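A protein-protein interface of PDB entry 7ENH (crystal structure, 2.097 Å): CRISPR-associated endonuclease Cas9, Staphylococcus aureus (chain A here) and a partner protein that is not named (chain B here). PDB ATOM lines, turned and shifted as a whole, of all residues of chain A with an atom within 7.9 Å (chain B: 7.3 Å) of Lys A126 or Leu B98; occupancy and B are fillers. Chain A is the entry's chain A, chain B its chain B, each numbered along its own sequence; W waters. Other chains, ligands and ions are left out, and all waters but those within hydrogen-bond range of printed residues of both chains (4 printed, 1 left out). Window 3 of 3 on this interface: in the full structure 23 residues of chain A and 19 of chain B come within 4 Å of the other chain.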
ATOM      1  N   LEU A  58       9.031  18.327   0.890  1.00  0.00           N
ATOM      2  CA  LEU A  58       9.744  19.032  -0.173  1.00  0.00           C
ATOM      3  C   LEU A  58      11.036  18.325  -0.571  1.00  0.00           C
ATOM      4  O   LEU A  58      11.933  18.940  -1.156  1.00  0.00           O
ATOM      5  CB  LEU A  58      10.021  20.490   0.210  1.00  0.00           C
ATOM      6  CG  LEU A  58       8.776  21.380   0.144  1.00  0.00           C
ATOM      7  CD1 LEU A  58       9.130  22.839   0.385  1.00  0.00           C
ATOM      8  CD2 LEU A  58       8.054  21.206  -1.186  1.00  0.00           C
ATOM      9  N   SER A 120       8.955  23.699   7.637  1.00  0.00           N
ATOM     10  CA  SER A 120       8.022  24.632   8.245  1.00  0.00           C
ATOM     11  C   SER A 120       6.803  24.828   7.349  1.00  0.00           C
ATOM     12  O   SER A 120       6.847  24.608   6.136  1.00  0.00           O
ATOM     13  CB  SER A 120       8.700  25.976   8.510  1.00  0.00           C
ATOM     14  OG  SER A 120       8.865  26.700   7.305  1.00  0.00           O
ATOM     15  N   TYR A 121       5.697  25.243   7.971  1.00  0.00           N
ATOM     16  CA  TYR A 121       4.502  25.559   7.197  1.00  0.00           C
ATOM     17  C   TYR A 121       4.723  26.772   6.306  1.00  0.00           C
ATOM     18  O   TYR A 121       4.096  26.888   5.247  1.00  0.00           O
ATOM     19  CB  TYR A 121       3.315  25.795   8.131  1.00  0.00           C
ATOM     20  CG  TYR A 121       2.045  26.181   7.408  1.00  0.00           C
ATOM     21  CD1 TYR A 121       1.346  25.250   6.652  1.00  0.00           C
ATOM     22  CD2 TYR A 121       1.551  27.477   7.474  1.00  0.00           C
ATOM     23  CE1 TYR A 121       0.186  25.598   5.985  1.00  0.00           C
ATOM     24  CE2 TYR A 121       0.391  27.834   6.811  1.00  0.00           C
ATOM     25  CZ  TYR A 121      -0.287  26.891   6.066  1.00  0.00           C
ATOM     26  OH  TYR A 121      -1.441  27.243   5.404  1.00  0.00           O
ATOM     27  N   GLU A 122       5.612  27.683   6.712  1.00  0.00           N
ATOM     28  CA  GLU A 122       5.896  28.860   5.896  1.00  0.00           C
ATOM     29  C   GLU A 122       6.596  28.474   4.600  1.00  0.00           C
ATOM     30  O   GLU A 122       6.242  28.963   3.521  1.00  0.00           O
ATOM     31  CB  GLU A 122       6.737  29.858   6.693  1.00  0.00           C
ATOM     32  CG  GLU A 122       5.978  30.548   7.812  1.00  0.00           C
ATOM     33  CD  GLU A 122       4.717  31.234   7.325  1.00  0.00           C
ATOM     34  OE1 GLU A 122       4.760  31.875   6.255  1.00  0.00           O
ATOM     35  OE2 GLU A 122       3.677  31.129   8.011  1.00  0.00           O
ATOM     36  N   THR A 123       7.600  27.598   4.686  1.00  0.00           N
ATOM     37  CA  THR A 123       8.235  27.081   3.478  1.00  0.00           C
ATOM     38  C   THR A 123       7.231  26.315   2.625  1.00  0.00           C
ATOM     39  O   THR A 123       7.209  26.457   1.396  1.00  0.00           O
ATOM     40  CB  THR A 123       9.415  26.182   3.848  1.00  0.00           C
ATOM     41  OG1 THR A 123      10.367  26.928   4.617  1.00  0.00           O
ATOM     42  CG2 THR A 123      10.094  25.643   2.597  1.00  0.00           C
ATOM     43  N   PHE A 124       6.385  25.509   3.268  1.00  0.00           N
ATOM     44  CA  PHE A 124       5.365  24.751   2.550  1.00  0.00           C
ATOM     45  C   PHE A 124       4.380  25.678   1.848  1.00  0.00           C
ATOM     46  O   PHE A 124       4.052  25.480   0.674  1.00  0.00           O
ATOM     47  CB  PHE A 124       4.647  23.822   3.530  1.00  0.00           C
ATOM     48  CG  PHE A 124       3.417  23.164   2.970  1.00  0.00           C
ATOM     49  CD1 PHE A 124       3.513  21.990   2.243  1.00  0.00           C
ATOM     50  CD2 PHE A 124       2.160  23.697   3.211  1.00  0.00           C
ATOM     51  CE1 PHE A 124       2.383  21.373   1.743  1.00  0.00           C
ATOM     52  CE2 PHE A 124       1.026  23.086   2.713  1.00  0.00           C
ATOM     53  CZ  PHE A 124       1.136  21.922   1.978  1.00  0.00           C
ATOM     54  N   LYS A 125       3.901  26.706   2.557  1.00  0.00           N
ATOM     55  CA  LYS A 125       2.917  27.614   1.974  1.00  0.00           C
ATOM     56  C   LYS A 125       3.497  28.375   0.788  1.00  0.00           C
ATOM     57  O   LYS A 125       2.832  28.529  -0.245  1.00  0.00           O
ATOM     58  CB  LYS A 125       2.408  28.586   3.038  1.00  0.00           C
ATOM     59  CG  LYS A 125       1.569  29.725   2.483  1.00  0.00           C
ATOM     60  CD  LYS A 125       1.155  30.695   3.578  1.00  0.00           C
ATOM     61  CE  LYS A 125      -0.125  30.243   4.259  1.00  0.00           C
ATOM     62  NZ  LYS A 125      -0.520  31.161   5.363  1.00  0.00           N
ATOM     63  N   LYS A 126       4.734  28.864   0.917  1.00  0.00           N
ATOM     64  CA  LYS A 126       5.368  29.574  -0.191  1.00  0.00           C
ATOM     65  C   LYS A 126       5.492  28.680  -1.419  1.00  0.00           C
ATOM     66  O   LYS A 126       5.270  29.130  -2.550  1.00  0.00           O
ATOM     67  CB  LYS A 126       6.741  30.093   0.237  1.00  0.00           C
ATOM     68  CG  LYS A 126       7.574  30.667  -0.899  1.00  0.00           C
ATOM     69  CD  LYS A 126       8.995  30.966  -0.448  1.00  0.00           C
ATOM     70  CE  LYS A 126       9.258  32.462  -0.398  1.00  0.00           C
ATOM     71  NZ  LYS A 126      10.654  32.766   0.025  1.00  0.00           N
ATOM     72  N   HIS A 127       5.835  27.407  -1.215  1.00  0.00           N
ATOM     73  CA  HIS A 127       5.957  26.484  -2.339  1.00  0.00           C
ATOM     74  C   HIS A 127       4.599  26.178  -2.956  1.00  0.00           C
ATOM     75  O   HIS A 127       4.478  26.071  -4.183  1.00  0.00           O
ATOM     76  CB  HIS A 127       6.641  25.196  -1.883  1.00  0.00           C
ATOM     77  CG  HIS A 127       6.960  24.253  -3.001  1.00  0.00           C
ATOM     78  ND1 HIS A 127       8.153  24.290  -3.690  1.00  0.00           N
ATOM     79  CD2 HIS A 127       6.239  23.246  -3.550  1.00  0.00           C
ATOM     80  CE1 HIS A 127       8.154  23.346  -4.615  1.00  0.00           C
ATOM     81  NE2 HIS A 127       7.005  22.699  -4.552  1.00  0.00           N
ATOM     82  N   ILE A 128       3.564  26.034  -2.125  1.00  0.00           N
ATOM     83  CA  ILE A 128       2.237  25.712  -2.640  1.00  0.00           C
ATOM     84  C   ILE A 128       1.662  26.889  -3.419  1.00  0.00           C
ATOM     85  O   ILE A 128       1.060  26.709  -4.485  1.00  0.00           O
ATOM     86  CB  ILE A 128       1.306  25.283  -1.491  1.00  0.00           C
ATOM     87  CG1 ILE A 128       1.775  23.953  -0.896  1.00  0.00           C
ATOM     88  CG2 ILE A 128      -0.133  25.175  -1.975  1.00  0.00           C
ATOM     89  CD1 ILE A 128       1.986  22.864  -1.923  1.00  0.00           C
ATOM     90  N   LEU A 129       1.839  28.109  -2.905  1.00  0.00           N
ATOM     91  CA  LEU A 129       1.333  29.287  -3.604  1.00  0.00           C
ATOM     92  C   LEU A 129       1.998  29.449  -4.965  1.00  0.00           C
ATOM     93  O   LEU A 129       1.336  29.792  -5.952  1.00  0.00           O
ATOM     94  CB  LEU A 129       1.543  30.536  -2.749  1.00  0.00           C
ATOM     95  CG  LEU A 129       0.645  30.682  -1.518  1.00  0.00           C
ATOM     96  CD1 LEU A 129       1.112  31.835  -0.643  1.00  0.00           C
ATOM     97  CD2 LEU A 129      -0.805  30.874  -1.934  1.00  0.00           C
ATOM     98  N   ASN A 130       3.308  29.202  -5.039  1.00  0.00           N
ATOM     99  CA  ASN A 130       3.999  29.271  -6.322  1.00  0.00           C
ATOM    100  C   ASN A 130       3.589  28.129  -7.241  1.00  0.00           C
ATOM    101  O   ASN A 130       3.512  28.315  -8.461  1.00  0.00           O
ATOM    102  CB  ASN A 130       5.512  29.263  -6.104  1.00  0.00           C
ATOM    103  CG  ASN A 130       6.286  29.111  -7.398  1.00  0.00           C
ATOM    104  OD1 ASN A 130       6.796  28.035  -7.706  1.00  0.00           O
ATOM    105  ND2 ASN A 130       6.376  30.192  -8.164  1.00  0.00           N
ATOM    106  N   LEU A 131       3.317  26.949  -6.678  1.00  0.00           N
ATOM    107  CA  LEU A 131       2.884  25.821  -7.495  1.00  0.00           C
ATOM    108  C   LEU A 131       1.517  26.072  -8.118  1.00  0.00           C
ATOM    109  O   LEU A 131       1.238  25.576  -9.216  1.00  0.00           O
ATOM    110  CB  LEU A 131       2.861  24.545  -6.652  1.00  0.00           C
ATOM    111  CG  LEU A 131       2.854  23.210  -7.397  1.00  0.00           C
ATOM    112  CD1 LEU A 131       4.093  23.069  -8.266  1.00  0.00           C
ATOM    113  CD2 LEU A 131       2.747  22.053  -6.415  1.00  0.00           C
ATOM    114  N   ALA A 132       0.662  26.840  -7.444  1.00  0.00           N
ATOM    115  CA  ALA A 132      -0.681  27.130  -7.938  1.00  0.00           C
ATOM    116  C   ALA A 132      -0.714  28.406  -8.776  1.00  0.00           C
ATOM    117  O   ALA A 132      -1.062  28.370  -9.960  1.00  0.00           O
ATOM    118  CB  ALA A 132      -1.660  27.236  -6.763  1.00  0.00           C
ATOM    119  N   LEU A 147      -3.661  24.599   2.159  1.00  0.00           N
ATOM    120  CA  LEU A 147      -3.480  25.745   3.039  1.00  0.00           C
ATOM    121  C   LEU A 147      -4.649  25.930   4.001  1.00  0.00           C
ATOM    122  O   LEU A 147      -4.878  27.045   4.482  1.00  0.00           O
ATOM    123  CB  LEU A 147      -3.262  27.013   2.212  1.00  0.00           C
ATOM    124  CG  LEU A 147      -2.109  26.930   1.208  1.00  0.00           C
ATOM    125  CD1 LEU A 147      -1.905  28.263   0.504  1.00  0.00           C
ATOM    126  CD2 LEU A 147      -0.825  26.479   1.893  1.00  0.00           C
ATOM    127  N   MET B  10       7.817  27.201  16.706  1.00  0.00           N
ATOM    128  CA  MET B  10       7.396  28.593  16.711  1.00  0.00           C
ATOM    129  C   MET B  10       7.606  29.189  15.327  1.00  0.00           C
ATOM    130  O   MET B  10       8.464  28.739  14.561  1.00  0.00           O
ATOM    131  CB  MET B  10       8.158  29.419  17.758  1.00  0.00           C
ATOM    132  CG  MET B  10       7.800  29.084  19.199  1.00  0.00           C
ATOM    133  SD  MET B  10       8.665  30.114  20.400  1.00  0.00           S
ATOM    134  CE  MET B  10       7.975  31.725  20.031  1.00  0.00           C
ATOM    135  N   SER B  11       6.808  30.207  15.013  1.00  0.00           N
ATOM    136  CA  SER B  11       6.911  30.902  13.735  1.00  0.00           C
ATOM    137  C   SER B  11       6.474  32.344  13.934  1.00  0.00           C
ATOM    138  O   SER B  11       5.346  32.594  14.372  1.00  0.00           O
ATOM    139  CB  SER B  11       6.054  30.223  12.665  1.00  0.00           C
ATOM    140  OG  SER B  11       6.090  30.946  11.447  1.00  0.00           O
ATOM    141  N   LYS B  12       7.360  33.284  13.617  1.00  0.00           N
ATOM    142  CA  LYS B  12       7.036  34.696  13.766  1.00  0.00           C
ATOM    143  C   LYS B  12       6.070  35.134  12.672  1.00  0.00           C
ATOM    144  O   LYS B  12       6.290  34.863  11.488  1.00  0.00           O
ATOM    145  CB  LYS B  12       8.306  35.544  13.721  1.00  0.00           C
ATOM    146  CG  LYS B  12       8.043  37.041  13.820  1.00  0.00           C
ATOM    147  CD  LYS B  12       9.218  37.781  14.440  1.00  0.00           C
ATOM    148  CE  LYS B  12      10.472  37.642  13.595  1.00  0.00           C
ATOM    149  NZ  LYS B  12      11.610  38.416  14.165  1.00  0.00           N
ATOM    150  N   GLN B  13       4.999  35.807  13.072  1.00  0.00           N
ATOM    151  CA  GLN B  13       4.010  36.348  12.154  1.00  0.00           C
ATOM    152  C   GLN B  13       4.007  37.870  12.254  1.00  0.00           C
ATOM    153  O   GLN B  13       4.740  38.465  13.049  1.00  0.00           O
ATOM    154  CB  GLN B  13       2.623  35.765  12.442  1.00  0.00           C
ATOM    155  CG  GLN B  13       2.592  34.242  12.476  1.00  0.00           C
ATOM    156  CD  GLN B  13       2.821  33.620  11.110  1.00  0.00           C
ATOM    157  OE1 GLN B  13       1.994  33.753  10.208  1.00  0.00           O
ATOM    158  NE2 GLN B  13       3.948  32.934  10.953  1.00  0.00           N
ATOM    159  N   ARG B  18       2.998  32.017  15.899  1.00  0.00           N
ATOM    160  CA  ARG B  18       2.393  30.692  15.920  1.00  0.00           C
ATOM    161  C   ARG B  18       3.217  29.798  16.836  1.00  0.00           C
ATOM    162  O   ARG B  18       4.442  29.726  16.705  1.00  0.00           O
ATOM    163  CB  ARG B  18       2.323  30.105  14.512  1.00  0.00           C
ATOM    164  CG  ARG B  18       1.811  28.675  14.459  1.00  0.00           C
ATOM    165  CD  ARG B  18       1.421  28.272  13.044  1.00  0.00           C
ATOM    166  NE  ARG B  18       2.522  28.433  12.098  1.00  0.00           N
ATOM    167  CZ  ARG B  18       2.505  29.267  11.063  1.00  0.00           C
ATOM    168  NH1 ARG B  18       1.439  30.023  10.833  1.00  0.00           N
ATOM    169  NH2 ARG B  18       3.555  29.348  10.257  1.00  0.00           N
ATOM    170  N   TYR B  74      14.845  22.439  15.146  1.00  0.00           N
ATOM    171  CA  TYR B  74      14.814  23.383  16.254  1.00  0.00           C
ATOM    172  C   TYR B  74      15.018  22.649  17.573  1.00  0.00           C
ATOM    173  O   TYR B  74      14.571  21.514  17.752  1.00  0.00           O
ATOM    174  CB  TYR B  74      13.480  24.134  16.292  1.00  0.00           C
ATOM    175  CG  TYR B  74      13.145  24.940  15.054  1.00  0.00           C
ATOM    176  CD1 TYR B  74      14.115  25.257  14.111  1.00  0.00           C
ATOM    177  CD2 TYR B  74      11.848  25.389  14.834  1.00  0.00           C
ATOM    178  CE1 TYR B  74      13.800  25.994  12.983  1.00  0.00           C
ATOM    179  CE2 TYR B  74      11.525  26.126  13.710  1.00  0.00           C
ATOM    180  CZ  TYR B  74      12.504  26.425  12.789  1.00  0.00           C
ATOM    181  OH  TYR B  74      12.186  27.158  11.670  1.00  0.00           O
ATOM    182  N   LYS B  93      18.201  29.170  12.706  1.00  0.00           N
ATOM    183  CA  LYS B  93      17.528  28.117  11.954  1.00  0.00           C
ATOM    184  C   LYS B  93      16.134  28.559  11.522  1.00  0.00           C
ATOM    185  O   LYS B  93      15.693  28.241  10.412  1.00  0.00           O
ATOM    186  CB  LYS B  93      17.458  26.841  12.786  1.00  0.00           C
ATOM    187  CG  LYS B  93      17.096  25.603  11.985  1.00  0.00           C
ATOM    188  CD  LYS B  93      17.627  24.347  12.652  1.00  0.00           C
ATOM    189  CE  LYS B  93      18.371  23.475  11.659  1.00  0.00           C
ATOM    190  NZ  LYS B  93      17.600  23.317  10.397  1.00  0.00           N
ATOM    191  N   MET B  94      15.424  29.300  12.381  1.00  0.00           N
ATOM    192  CA  MET B  94      14.098  29.792  12.013  1.00  0.00           C
ATOM    193  C   MET B  94      14.167  30.765  10.843  1.00  0.00           C
ATOM    194  O   MET B  94      13.232  30.829  10.038  1.00  0.00           O
ATOM    195  CB  MET B  94      13.428  30.455  13.215  1.00  0.00           C
ATOM    196  CG  MET B  94      12.979  29.479  14.289  1.00  0.00           C
ATOM    197  SD  MET B  94      12.692  30.279  15.880  1.00  0.00           S
ATOM    198  CE  MET B  94      11.210  31.219  15.523  1.00  0.00           C
ATOM    199  N   LYS B  95      15.263  31.523  10.730  1.00  0.00           N
ATOM    200  CA  LYS B  95      15.409  32.447   9.610  1.00  0.00           C
ATOM    201  C   LYS B  95      15.474  31.699   8.283  1.00  0.00           C
ATOM    202  O   LYS B  95      14.897  32.141   7.281  1.00  0.00           O
ATOM    203  CB  LYS B  95      16.661  33.306   9.795  1.00  0.00           C
ATOM    204  CG  LYS B  95      16.489  34.465  10.765  1.00  0.00           C
ATOM    205  CD  LYS B  95      17.794  34.772  11.483  1.00  0.00           C
ATOM    206  CE  LYS B  95      17.805  36.194  12.018  1.00  0.00           C
ATOM    207  NZ  LYS B  95      19.176  36.623  12.407  1.00  0.00           N
ATOM    208  N   GLU B  96      16.168  30.558   8.263  1.00  0.00           N
ATOM    209  CA  GLU B  96      16.305  29.773   7.042  1.00  0.00           C
ATOM    210  C   GLU B  96      15.022  29.039   6.674  1.00  0.00           C
ATOM    211  O   GLU B  96      14.836  28.693   5.505  1.00  0.00           O
ATOM    212  CB  GLU B  96      17.463  28.780   7.194  1.00  0.00           C
ATOM    213  CG  GLU B  96      18.743  29.416   7.713  1.00  0.00           C
ATOM    214  CD  GLU B  96      19.923  28.468   7.680  1.00  0.00           C
ATOM    215  OE1 GLU B  96      21.069  28.959   7.706  1.00  0.00           O
ATOM    216  OE2 GLU B  96      19.710  27.237   7.624  1.00  0.00           O
ATOM    217  N   ASN B  97      14.128  28.813   7.636  1.00  0.00           N
ATOM    218  CA  ASN B  97      12.842  28.176   7.383  1.00  0.00           C
ATOM    219  C   ASN B  97      11.695  29.180   7.347  1.00  0.00           C
ATOM    220  O   ASN B  97      10.536  28.793   7.534  1.00  0.00           O
ATOM    221  CB  ASN B  97      12.567  27.101   8.435  1.00  0.00           C
ATOM    222  CG  ASN B  97      13.595  25.988   8.418  1.00  0.00           C
ATOM    223  OD1 ASN B  97      14.497  25.942   9.256  1.00  0.00           O
ATOM    224  ND2 ASN B  97      13.466  25.083   7.456  1.00  0.00           N
ATOM    225  N   LEU B  98      12.003  30.460   7.128  1.00  0.00           N
ATOM    226  CA  LEU B  98      11.002  31.521   7.003  1.00  0.00           C
ATOM    227  C   LEU B  98      10.139  31.650   8.257  1.00  0.00           C
ATOM    228  O   LEU B  98       8.979  32.063   8.183  1.00  0.00           O
ATOM    229  CB  LEU B  98      10.122  31.310   5.768  1.00  0.00           C
ATOM    230  CG  LEU B  98      10.857  31.206   4.431  1.00  0.00           C
ATOM    231  CD1 LEU B  98       9.910  30.745   3.334  1.00  0.00           C
ATOM    232  CD2 LEU B  98      11.499  32.536   4.066  1.00  0.00           C
ATOM    233  N   ASP B  99      10.695  31.303   9.415  1.00  0.00           N
ATOM    234  CA  ASP B  99       9.988  31.414  10.683  1.00  0.00           C
ATOM    235  C   ASP B  99      10.469  32.587  11.527  1.00  0.00           C
ATOM    236  O   ASP B  99       9.992  32.759  12.653  1.00  0.00           O
ATOM    237  CB  ASP B  99      10.127  30.114  11.483  1.00  0.00           C
ATOM    238  CG  ASP B  99       9.294  28.987  10.908  1.00  0.00           C
ATOM    239  OD1 ASP B  99       8.223  29.272  10.333  1.00  0.00           O
ATOM    240  OD2 ASP B  99       9.712  27.817  11.034  1.00  0.00           O
ATOM    241  N   TYR B 100      11.394  33.392  11.015  1.00  0.00           N
ATOM    242  CA  TYR B 100      11.917  34.532  11.757  1.00  0.00           C
ATOM    243  C   TYR B 100      12.424  35.610  10.807  1.00  0.00           C
ATOM    244  O   TYR B 100      13.106  35.314   9.825  1.00  0.00           O
ATOM    245  CB  TYR B 100      13.037  34.092  12.701  1.00  0.00           C
ATOM    246  CG  TYR B 100      13.353  35.095  13.786  1.00  0.00           C
ATOM    247  CD1 TYR B 100      12.674  35.073  14.998  1.00  0.00           C
ATOM    248  CD2 TYR B 100      14.328  36.066  13.599  1.00  0.00           C
ATOM    249  CE1 TYR B 100      12.959  35.989  15.992  1.00  0.00           C
ATOM    250  CE2 TYR B 100      14.618  36.988  14.586  1.00  0.00           C
ATOM    251  CZ  TYR B 100      13.932  36.943  15.782  1.00  0.00           C
ATOM    252  OH  TYR B 100      14.218  37.857  16.770  1.00  0.00           O
HETATM  253  O   HOH W   1      12.465  27.976   3.287  1.00  0.00           O
HETATM  254  O   HOH W   2       7.350  33.500   6.943  1.00  0.00           O
HETATM  255  O   HOH W   3      11.379  24.823   6.287  1.00  0.00           O
HETATM  256  O   HOH W   4       0.912  31.808   8.292  1.00  0.00           O
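The side-chain hydroxyl (OG) of Ser A120 is in hydrogen-bond range of the backbone carbonyl oxygen (O) of Asn B97, at 2.7 Å.
OE2 of Glu A122 is in salt-bridge range of NH2 of Arg B18 (2.9 Å).
The side-chain amide nitrogen (NE2) of Gln B13 is in hydrogen-bond range of the side-chain carboxylate (OE2) of Glu A122 (3.5 Å).
OG1 of Thr A123 lies within hydrogen-bond range of O of Asn B97, 3.5 Å away.
O of Met B94 sits at hydrogen-bond distance from N of Asp B99, 2.7 Å away.
The side-chain hydroxyl of Ser B11 lies within hydrogen-bond range of the side-chain amide nitrogen of Gln B13, 3.0 Å away.
The side-chain hydroxyl of Ser A120 lies close to the backbone NH of Glu A122 (3.4 Å).
OD2 of Asp B99 lies within hydrogen-bond range of OH of Tyr B74, 2.6 Å away.
OG of Ser A120 sits at hydrogen-bond distance from N of Thr A123 (3.0 Å).
O of Asp B99 lies within hydrogen-bond range of N of Lys B12.
Asp B99 touches Ser A120 (OD2 to CB, 3.3 Å).
Arg B18 touches Tyr A121 (NH2 to CD2, 3.9 Å).
Glu A122 touches Ser B11 (CG to OG, 3.7 Å).
Leu B98 touches Glu A122 (O to CG, 3.4 Å).
Glu A122 touches Asp B99 (CG to OD1, 3.6 Å).
CD1 of Leu B98 touches CD of Lys A126, at 3.9 Å.
Of chain B, only Leu B98 comes within 4 Å of Lys A126.
Leu B98 touches just these residues of chain A: Glu A122 (3.4 Å) and Lys A126 (3.9 Å).
Of the printed residues of chain B, Ser A120 touches Asn B97 (2.7 Å) and Asp B99 (3.3 Å).
Printed residues of chain A within 4 Å of Asn B97: Ser A120 and Thr A123.
Of the printed residues of chain B, Tyr A121 touches Arg B18.
Of the printed residues of chain B, Thr A123 touches Asn B97.
Printed residues of chain A within 4 Å of Arg B18: Tyr A121 and Glu A122.
Lys B93 touches none of the printed residues of chain A.
Leu A147 touches none of the printed residues of chain B.
The nearest printed residue of chain A that does not touch Asn B97 is Glu A122 (4.03 Å).
Of the 15 printed residues of chain A, 5 touch a printed residue of chain B.
Printed residues of chain B that touch a printed residue of chain A: Ser B11, Gln B13, Arg B18, Asn B97, Leu B98 and Asp B99.
Hydrophobic or aromatic side chains of chain B that line the printed part of chain A: Leu B98.
Among the printed residues, Asp or Glu carboxylates within 4 Å of a Lys or Arg side-chain nitrogen of the other chain: Glu A122 with Arg B18.
Water W3 lies within hydrogen-bond range of the side-chain amide nitrogen (ND2) of Asn B97 (2.4 Å), the side-chain hydroxyl (OG1) of Thr A123 (2.9 Å) and the backbone NH (N) of Ser A120 (3.0 Å).
Water W2 lies within hydrogen-bond range of O of Leu B98 (2.5 Å) and OE1 of Glu A122 (3.1 Å).
Water W1 bridges OG1 of Thr A123 (2.7 Å) and O of Glu B96 (3.3 Å).
Water W4 lies within hydrogen-bond range of the side-chain carboxylate of Glu A122, the side-chain amide oxygen of Gln B13, the guanidinium group of Arg B18 and the side-chain amino group of Lys A125.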
